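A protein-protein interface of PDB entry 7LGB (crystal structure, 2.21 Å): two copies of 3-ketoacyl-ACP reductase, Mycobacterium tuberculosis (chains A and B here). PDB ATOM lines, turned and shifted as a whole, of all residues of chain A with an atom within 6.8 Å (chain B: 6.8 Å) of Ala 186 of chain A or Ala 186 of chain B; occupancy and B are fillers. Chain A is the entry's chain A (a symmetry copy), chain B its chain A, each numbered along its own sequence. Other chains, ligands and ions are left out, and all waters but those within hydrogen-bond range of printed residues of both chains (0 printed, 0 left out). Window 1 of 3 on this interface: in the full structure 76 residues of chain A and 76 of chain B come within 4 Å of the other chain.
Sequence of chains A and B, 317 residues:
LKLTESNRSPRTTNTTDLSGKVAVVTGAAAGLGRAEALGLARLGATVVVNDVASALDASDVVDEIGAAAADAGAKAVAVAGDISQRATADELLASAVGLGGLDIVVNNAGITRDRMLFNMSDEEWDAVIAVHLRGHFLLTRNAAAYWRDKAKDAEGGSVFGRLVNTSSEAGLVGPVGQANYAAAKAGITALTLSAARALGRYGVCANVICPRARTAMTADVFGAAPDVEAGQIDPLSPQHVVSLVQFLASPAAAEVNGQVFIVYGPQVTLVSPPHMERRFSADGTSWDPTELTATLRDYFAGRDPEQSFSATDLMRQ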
ATOM      1  N   LEU A 133      37.249  12.641  14.899  1.00  0.00           N
ATOM      2  CA  LEU A 133      36.450  13.314  15.912  1.00  0.00           C
ATOM      3  C   LEU A 133      37.242  14.410  16.605  1.00  0.00           C
ATOM      4  O   LEU A 133      36.767  15.551  16.707  1.00  0.00           O
ATOM      5  CB  LEU A 133      35.920  12.302  16.932  1.00  0.00           C
ATOM      6  CG  LEU A 133      34.899  12.882  17.916  1.00  0.00           C
ATOM      7  CD1 LEU A 133      33.785  13.670  17.184  1.00  0.00           C
ATOM      8  CD2 LEU A 133      34.301  11.754  18.779  1.00  0.00           C
ATOM      9  N   SER A 167      30.338  13.917   8.102  1.00  0.00           N
ATOM     10  CA  SER A 167      29.951  12.692   8.769  1.00  0.00           C
ATOM     11  C   SER A 167      29.867  11.590   7.717  1.00  0.00           C
ATOM     12  O   SER A 167      30.548  11.643   6.682  1.00  0.00           O
ATOM     13  CB  SER A 167      28.615  12.892   9.504  1.00  0.00           C
ATOM     14  OG  SER A 167      28.254  11.770  10.299  1.00  0.00           O
ATOM     15  N   SER A 168      29.025  10.595   7.956  1.00  0.00           N
ATOM     16  CA  SER A 168      28.878   9.502   7.011  1.00  0.00           C
ATOM     17  C   SER A 168      27.605   8.757   7.367  1.00  0.00           C
ATOM     18  O   SER A 168      27.202   8.729   8.536  1.00  0.00           O
ATOM     19  CB  SER A 168      30.089   8.553   7.055  1.00  0.00           C
ATOM     20  OG  SER A 168      29.809   7.331   6.398  1.00  0.00           O
ATOM     21  N   ALA A 170      27.623   5.767   7.600  1.00  0.00           N
ATOM     22  CA  ALA A 170      28.089   4.767   8.558  1.00  0.00           C
ATOM     23  C   ALA A 170      27.784   5.190   9.990  1.00  0.00           C
ATOM     24  O   ALA A 170      27.560   4.338  10.858  1.00  0.00           O
ATOM     25  CB  ALA A 170      29.590   4.514   8.386  1.00  0.00           C
ATOM     26  N   GLY A 171      27.754   6.495  10.255  1.00  0.00           N
ATOM     27  CA  GLY A 171      27.436   6.962  11.590  1.00  0.00           C
ATOM     28  C   GLY A 171      25.977   6.822  11.952  1.00  0.00           C
ATOM     29  O   GLY A 171      25.630   6.932  13.132  1.00  0.00           O
ATOM     30  N   LEU A 172      25.117   6.585  10.967  1.00  0.00           N
ATOM     31  CA  LEU A 172      23.706   6.359  11.228  1.00  0.00           C
ATOM     32  C   LEU A 172      23.379   4.886  11.382  1.00  0.00           C
ATOM     33  O   LEU A 172      22.303   4.554  11.887  1.00  0.00           O
ATOM     34  CB  LEU A 172      22.854   6.940  10.087  1.00  0.00           C
ATOM     35  CG  LEU A 172      23.095   8.376   9.605  1.00  0.00           C
ATOM     36  CD1 LEU A 172      22.304   8.643   8.321  1.00  0.00           C
ATOM     37  CD2 LEU A 172      22.752   9.429  10.671  1.00  0.00           C
ATOM     38  N   TYR A 181      35.049   3.950  12.858  1.00  0.00           N
ATOM     39  CA  TYR A 181      34.636   4.953  11.884  1.00  0.00           C
ATOM     40  C   TYR A 181      33.216   5.445  12.164  1.00  0.00           C
ATOM     41  O   TYR A 181      32.947   6.653  12.154  1.00  0.00           O
ATOM     42  CB  TYR A 181      34.750   4.338  10.488  1.00  0.00           C
ATOM     43  CG  TYR A 181      34.469   5.272   9.331  1.00  0.00           C
ATOM     44  CD1 TYR A 181      35.440   6.135   8.866  1.00  0.00           C
ATOM     45  CD2 TYR A 181      33.249   5.247   8.675  1.00  0.00           C
ATOM     46  CE1 TYR A 181      35.201   6.981   7.792  1.00  0.00           C
ATOM     47  CE2 TYR A 181      32.998   6.081   7.589  1.00  0.00           C
ATOM     48  CZ  TYR A 181      33.977   6.946   7.161  1.00  0.00           C
ATOM     49  OH  TYR A 181      33.740   7.777   6.093  1.00  0.00           O
ATOM     50  N   ALA A 182      32.289   4.516  12.413  1.00  0.00           N
ATOM     51  CA  ALA A 182      30.905   4.902  12.685  1.00  0.00           C
ATOM     52  C   ALA A 182      30.798   5.762  13.944  1.00  0.00           C
ATOM     53  O   ALA A 182      30.060   6.754  13.975  1.00  0.00           O
ATOM     54  CB  ALA A 182      30.040   3.651  12.829  1.00  0.00           C
ATOM     55  N   ALA A 183      31.513   5.380  15.001  1.00  0.00           N
ATOM     56  CA  ALA A 183      31.466   6.149  16.238  1.00  0.00           C
ATOM     57  C   ALA A 183      31.978   7.571  16.023  1.00  0.00           C
ATOM     58  O   ALA A 183      31.363   8.534  16.490  1.00  0.00           O
ATOM     59  CB  ALA A 183      32.271   5.433  17.323  1.00  0.00           C
ATOM     60  N   ALA A 184      33.081   7.725  15.286  1.00  0.00           N
ATOM     61  CA  ALA A 184      33.621   9.059  15.021  1.00  0.00           C
ATOM     62  C   ALA A 184      32.650   9.908  14.208  1.00  0.00           C
ATOM     63  O   ALA A 184      32.447  11.089  14.502  1.00  0.00           O
ATOM     64  CB  ALA A 184      34.961   8.943  14.291  1.00  0.00           C
ATOM     65  N   LYS A 185      32.043   9.329  13.175  1.00  0.00           N
ATOM     66  CA  LYS A 185      31.166  10.109  12.314  1.00  0.00           C
ATOM     67  C   LYS A 185      29.892  10.516  13.037  1.00  0.00           C
ATOM     68  O   LYS A 185      29.392  11.627  12.830  1.00  0.00           O
ATOM     69  CB  LYS A 185      30.831   9.328  11.041  1.00  0.00           C
ATOM     70  CG  LYS A 185      32.027   9.143  10.101  1.00  0.00           C
ATOM     71  CD  LYS A 185      32.776  10.439   9.932  1.00  0.00           C
ATOM     72  CE  LYS A 185      33.555  10.461   8.623  1.00  0.00           C
ATOM     73  NZ  LYS A 185      34.135  11.825   8.385  1.00  0.00           N
ATOM     74  N   ALA A 186      29.334   9.621  13.862  1.00  0.00           N
ATOM     75  CA  ALA A 186      28.171   9.985  14.669  1.00  0.00           C
ATOM     76  C   ALA A 186      28.521  11.086  15.665  1.00  0.00           C
ATOM     77  O   ALA A 186      27.766  12.053  15.819  1.00  0.00           O
ATOM     78  CB  ALA A 186      27.609   8.756  15.399  1.00  0.00           C
ATOM     79  N   GLY A 187      29.670  10.965  16.339  1.00  0.00           N
ATOM     80  CA  GLY A 187      30.120  12.048  17.213  1.00  0.00           C
ATOM     81  C   GLY A 187      30.234  13.380  16.490  1.00  0.00           C
ATOM     82  O   GLY A 187      29.816  14.419  17.010  1.00  0.00           O
ATOM     83  N   ILE A 188      30.790  13.359  15.274  1.00  0.00           N
ATOM     84  CA  ILE A 188      30.939  14.565  14.461  1.00  0.00           C
ATOM     85  C   ILE A 188      29.586  15.233  14.240  1.00  0.00           C
ATOM     86  O   ILE A 188      29.455  16.460  14.335  1.00  0.00           O
ATOM     87  CB  ILE A 188      31.620  14.218  13.119  1.00  0.00           C
ATOM     88  CG1 ILE A 188      33.133  14.059  13.308  1.00  0.00           C
ATOM     89  CG2 ILE A 188      31.294  15.275  12.056  1.00  0.00           C
ATOM     90  CD1 ILE A 188      33.834  13.320  12.180  1.00  0.00           C
ATOM     91  N   THR A 189      28.559  14.437  13.952  1.00  0.00           N
ATOM     92  CA  THR A 189      27.230  14.998  13.736  1.00  0.00           C
ATOM     93  C   THR A 189      26.733  15.727  14.978  1.00  0.00           C
ATOM     94  O   THR A 189      26.301  16.885  14.904  1.00  0.00           O
ATOM     95  CB  THR A 189      26.282  13.872  13.334  1.00  0.00           C
ATOM     96  OG1 THR A 189      26.673  13.408  12.046  1.00  0.00           O
ATOM     97  CG2 THR A 189      24.814  14.334  13.304  1.00  0.00           C
ATOM     98  N   ALA A 190      26.816  15.064  16.140  1.00  0.00           N
ATOM     99  CA  ALA A 190      26.348  15.670  17.383  1.00  0.00           C
ATOM    100  C   ALA A 190      27.175  16.896  17.741  1.00  0.00           C
ATOM    101  O   ALA A 190      26.630  17.905  18.210  1.00  0.00           O
ATOM    102  CB  ALA A 190      26.384  14.637  18.518  1.00  0.00           C
ATOM    103  N   LEU A 191      28.495  16.830  17.520  1.00  0.00           N
ATOM    104  CA  LEU A 191      29.354  17.998  17.709  1.00  0.00           C
ATOM    105  C   LEU A 191      28.871  19.182  16.880  1.00  0.00           C
ATOM    106  O   LEU A 191      28.821  20.322  17.364  1.00  0.00           O
ATOM    107  CB  LEU A 191      30.805  17.658  17.332  1.00  0.00           C
ATOM    108  CG  LEU A 191      31.711  18.843  16.951  1.00  0.00           C
ATOM    109  CD1 LEU A 191      32.017  19.752  18.152  1.00  0.00           C
ATOM    110  CD2 LEU A 191      33.001  18.391  16.283  1.00  0.00           C
ATOM    111  N   LEU B 133      33.150   7.321  25.685  1.00  0.00           N
ATOM    112  CA  LEU B 133      33.279   6.632  24.410  1.00  0.00           C
ATOM    113  C   LEU B 133      34.374   5.580  24.456  1.00  0.00           C
ATOM    114  O   LEU B 133      34.141   4.423  24.077  1.00  0.00           O
ATOM    115  CB  LEU B 133      33.541   7.637  23.285  1.00  0.00           C
ATOM    116  CG  LEU B 133      33.484   7.033  21.879  1.00  0.00           C
ATOM    117  CD1 LEU B 133      32.202   6.189  21.673  1.00  0.00           C
ATOM    118  CD2 LEU B 133      33.585   8.149  20.821  1.00  0.00           C
ATOM    119  N   SER B 167      23.520   5.659  26.007  1.00  0.00           N
ATOM    120  CA  SER B 167      23.640   6.878  25.235  1.00  0.00           C
ATOM    121  C   SER B 167      22.820   7.959  25.933  1.00  0.00           C
ATOM    122  O   SER B 167      22.619   7.917  27.156  1.00  0.00           O
ATOM    123  CB  SER B 167      23.167   6.636  23.792  1.00  0.00           C
ATOM    124  OG  SER B 167      23.396   7.755  22.945  1.00  0.00           O
ATOM    125  N   SER B 168      22.325   8.923  25.171  1.00  0.00           N
ATOM    126  CA  SER B 168      21.531   9.994  25.747  1.00  0.00           C
ATOM    127  C   SER B 168      20.809  10.693  24.610  1.00  0.00           C
ATOM    128  O   SER B 168      21.305  10.722  23.478  1.00  0.00           O
ATOM    129  CB  SER B 168      22.411  10.991  26.521  1.00  0.00           C
ATOM    130  OG  SER B 168      21.711  12.190  26.795  1.00  0.00           O
ATOM    131  N   ALA B 170      20.860  13.684  24.404  1.00  0.00           N
ATOM    132  CA  ALA B 170      21.811  14.717  24.000  1.00  0.00           C
ATOM    133  C   ALA B 170      22.576  14.305  22.749  1.00  0.00           C
ATOM    134  O   ALA B 170      22.967  15.160  21.946  1.00  0.00           O
ATOM    135  CB  ALA B 170      22.785  15.028  25.142  1.00  0.00           C
ATOM    136  N   GLY B 171      22.787  13.004  22.555  1.00  0.00           N
ATOM    137  CA  GLY B 171      23.479  12.546  21.366  1.00  0.00           C
ATOM    138  C   GLY B 171      22.648  12.633  20.108  1.00  0.00           C
ATOM    139  O   GLY B 171      23.199  12.527  19.008  1.00  0.00           O
ATOM    140  N   LEU B 172      21.340  12.819  20.244  1.00  0.00           N
ATOM    141  CA  LEU B 172      20.473  12.991  19.091  1.00  0.00           C
ATOM    142  C   LEU B 172      20.278  14.453  18.732  1.00  0.00           C
ATOM    143  O   LEU B 172      19.818  14.749  17.626  1.00  0.00           O
ATOM    144  CB  LEU B 172      19.098  12.359  19.359  1.00  0.00           C
ATOM    145  CG  LEU B 172      19.005  10.926  19.901  1.00  0.00           C
ATOM    146  CD1 LEU B 172      17.564  10.607  20.310  1.00  0.00           C
ATOM    147  CD2 LEU B 172      19.519   9.877  18.902  1.00  0.00           C
ATOM    148  N   TYR B 181      29.801  15.882  25.553  1.00  0.00           N
ATOM    149  CA  TYR B 181      28.878  14.848  26.004  1.00  0.00           C
ATOM    150  C   TYR B 181      28.045  14.304  24.843  1.00  0.00           C
ATOM    151  O   TYR B 181      27.890  13.086  24.687  1.00  0.00           O
ATOM    152  CB  TYR B 181      27.988  15.445  27.097  1.00  0.00           C
ATOM    153  CG  TYR B 181      27.035  14.482  27.770  1.00  0.00           C
ATOM    154  CD1 TYR B 181      27.467  13.653  28.785  1.00  0.00           C
ATOM    155  CD2 TYR B 181      25.694  14.448  27.424  1.00  0.00           C
ATOM    156  CE1 TYR B 181      26.597  12.781  29.425  1.00  0.00           C
ATOM    157  CE2 TYR B 181      24.807  13.588  28.065  1.00  0.00           C
ATOM    158  CZ  TYR B 181      25.269  12.756  29.057  1.00  0.00           C
ATOM    159  OH  TYR B 181      24.405  11.899  29.693  1.00  0.00           O
ATOM    160  N   ALA B 182      27.497  15.198  24.017  1.00  0.00           N
ATOM    161  CA  ALA B 182      26.683  14.761  22.884  1.00  0.00           C
ATOM    162  C   ALA B 182      27.493  13.918  21.900  1.00  0.00           C
ATOM    163  O   ALA B 182      27.012  12.897  21.392  1.00  0.00           O
ATOM    164  CB  ALA B 182      26.095  15.978  22.171  1.00  0.00           C
ATOM    165  N   ALA B 183      28.719  14.345  21.603  1.00  0.00           N
ATOM    166  CA  ALA B 183      29.555  13.594  20.674  1.00  0.00           C
ATOM    167  C   ALA B 183      29.842  12.190  21.203  1.00  0.00           C
ATOM    168  O   ALA B 183      29.747  11.211  20.458  1.00  0.00           O
ATOM    169  CB  ALA B 183      30.854  14.359  20.413  1.00  0.00           C
ATOM    170  N   ALA B 184      30.158  12.070  22.495  1.00  0.00           N
ATOM    171  CA  ALA B 184      30.428  10.755  23.077  1.00  0.00           C
ATOM    172  C   ALA B 184      29.198   9.854  23.029  1.00  0.00           C
ATOM    173  O   ALA B 184      29.296   8.671  22.694  1.00  0.00           O
ATOM    174  CB  ALA B 184      30.910  10.913  24.520  1.00  0.00           C
ATOM    175  N   LYS B 185      28.029  10.392  23.366  1.00  0.00           N
ATOM    176  CA  LYS B 185      26.833   9.564  23.415  1.00  0.00           C
ATOM    177  C   LYS B 185      26.406   9.117  22.026  1.00  0.00           C
ATOM    178  O   LYS B 185      25.943   7.983  21.857  1.00  0.00           O
ATOM    179  CB  LYS B 185      25.692  10.310  24.111  1.00  0.00           C
ATOM    180  CG  LYS B 185      25.923  10.528  25.610  1.00  0.00           C
ATOM    181  CD  LYS B 185      26.410   9.261  26.262  1.00  0.00           C
ATOM    182  CE  LYS B 185      26.094   9.250  27.753  1.00  0.00           C
ATOM    183  NZ  LYS B 185      26.413   7.907  28.342  1.00  0.00           N
ATOM    184  N   ALA B 186      26.520  10.002  21.028  1.00  0.00           N
ATOM    185  CA  ALA B 186      26.229   9.604  19.652  1.00  0.00           C
ATOM    186  C   ALA B 186      27.206   8.534  19.176  1.00  0.00           C
ATOM    187  O   ALA B 186      26.796   7.540  18.565  1.00  0.00           O
ATOM    188  CB  ALA B 186      26.263  10.820  18.714  1.00  0.00           C
ATOM    189  N   GLY B 187      28.501   8.712  19.458  1.00  0.00           N
ATOM    190  CA  GLY B 187      29.468   7.662  19.139  1.00  0.00           C
ATOM    191  C   GLY B 187      29.115   6.324  19.768  1.00  0.00           C
ATOM    192  O   GLY B 187      29.203   5.277  19.119  1.00  0.00           O
ATOM    193  N   ILE B 188      28.697   6.348  21.038  1.00  0.00           N
ATOM    194  CA  ILE B 188      28.303   5.136  21.755  1.00  0.00           C
ATOM    195  C   ILE B 188      27.188   4.411  21.010  1.00  0.00           C
ATOM    196  O   ILE B 188      27.206   3.182  20.871  1.00  0.00           O
ATOM    197  CB  ILE B 188      27.878   5.490  23.197  1.00  0.00           C
ATOM    198  CG1 ILE B 188      29.109   5.713  24.083  1.00  0.00           C
ATOM    199  CG2 ILE B 188      26.960   4.403  23.773  1.00  0.00           C
ATOM    200  CD1 ILE B 188      28.828   6.462  25.375  1.00  0.00           C
ATOM    201  N   THR B 189      26.208   5.160  20.512  1.00  0.00           N
ATOM    202  CA  THR B 189      25.109   4.543  19.777  1.00  0.00           C
ATOM    203  C   THR B 189      25.617   3.814  18.540  1.00  0.00           C
ATOM    204  O   THR B 189      25.295   2.638  18.319  1.00  0.00           O
ATOM    205  CB  THR B 189      24.095   5.623  19.411  1.00  0.00           C
ATOM    206  OG1 THR B 189      23.489   6.082  20.615  1.00  0.00           O
ATOM    207  CG2 THR B 189      23.016   5.102  18.445  1.00  0.00           C
ATOM    208  N   ALA B 190      26.439   4.498  17.733  1.00  0.00           N
ATOM    209  CA  ALA B 190      26.963   3.893  16.511  1.00  0.00           C
ATOM    210  C   ALA B 190      27.863   2.707  16.829  1.00  0.00           C
ATOM    211  O   ALA B 190      27.822   1.685  16.131  1.00  0.00           O
ATOM    212  CB  ALA B 190      27.718   4.945  15.686  1.00  0.00           C
ATOM    213  N   LEU B 191      28.678   2.823  17.886  1.00  0.00           N
ATOM    214  CA  LEU B 191      29.484   1.694  18.348  1.00  0.00           C
ATOM    215  C   LEU B 191      28.615   0.479  18.648  1.00  0.00           C
ATOM    216  O   LEU B 191      28.953  -0.655  18.277  1.00  0.00           O
ATOM    217  CB  LEU B 191      30.278   2.087  19.605  1.00  0.00           C
ATOM    218  CG  LEU B 191      30.732   0.933  20.518  1.00  0.00           C
ATOM    219  CD1 LEU B 191      31.808   0.057  19.859  1.00  0.00           C
ATOM    220  CD2 LEU B 191      31.206   1.427  21.877  1.00  0.00           C
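Ala 182 of chain A touches Ala 190 of chain B, and with the chains exchanged Ala 190 of chain A touches Ala 182 of chain B. Ala 183 of chain A touches Gly 187 of chain B, and with the chains exchanged Gly 187 of chain A touches Ala 183 of chain B. Ala 183 of chain A touches Ala 190 of chain B, and with the chains exchanged Ala 190 of chain A touches Ala 183 of chain B. Ala 186 of chain A touches Ala 190 of chain B, and with the chains exchanged Ala 190 of chain A touches Ala 186 of chain B. Of the 11 pairs that touch across the chains among the printed residues, 11 have their exchanged pair printed and touching as well.
O of Gly 171 of chain A touches CB of Ala 190 of chain B, 3.9 Å away. O of Ala 182 of chain A touches CB of Ala 190 of chain B (3.4 Å). Ala 183 of chain A touches Gly 187 of chain B (O to CA, 3.4 Å). CB of Ala 190 of chain B touches N of Ala 183 of chain A, at 3.9 Å. CB of Ala 186 of chain B touches O of Ala 186 of chain A, at 3.5 Å. Gly 187 of chain A touches Ala 183 of chain B. Gly 171 of chain B touches Ala 190 of chain A. Ala 182 of chain B touches Ala 190 of chain A (O to CB, 3.4 Å). Ala 190 of chain A touches Ala 183 of chain B. Ala 190 of chain A touches Ala 186 of chain B (CB to CB, 3.8 Å).
Of the 17 printed residues of chain B, 6 touch a printed residue of chain A. Printed residues of chain B that touch a printed residue of chain A: Gly 171, Ala 182, Ala 183, Ala 186, Gly 187 and Ala 190. Hydrophobic or aromatic side chains of chain B that line the printed part of chain A: Ala 182, Ala 183, Ala 186 and Ala 190. Among the printed residues, 11 pairs touch across the chains. Among the printed residues, no Asp or Glu carboxylate lies within 4 Å of a Lys or Arg side-chain nitrogen of the other chain.
Of chain B, only Ala 186 (3.5 Å) and Ala 190 (3.8 Å) come within 4 Å of Ala 186 of chain A. Of chain A, only Ala 186 (3.5 Å) and Ala 190 (3.8 Å) come within 4 Å of Ala 186 of chain B. Printed residues of chain B within 4 Å of Gly 171 of chain A: Ala 190 (3.9 Å). Printed residues of chain B within 4 Å of Ala 182 of chain A: Ala 190. Of the printed residues of chain A, Gly 187 of chain B touches Ala 183. Leu 133 of chain A touches none of the printed residues of chain B.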
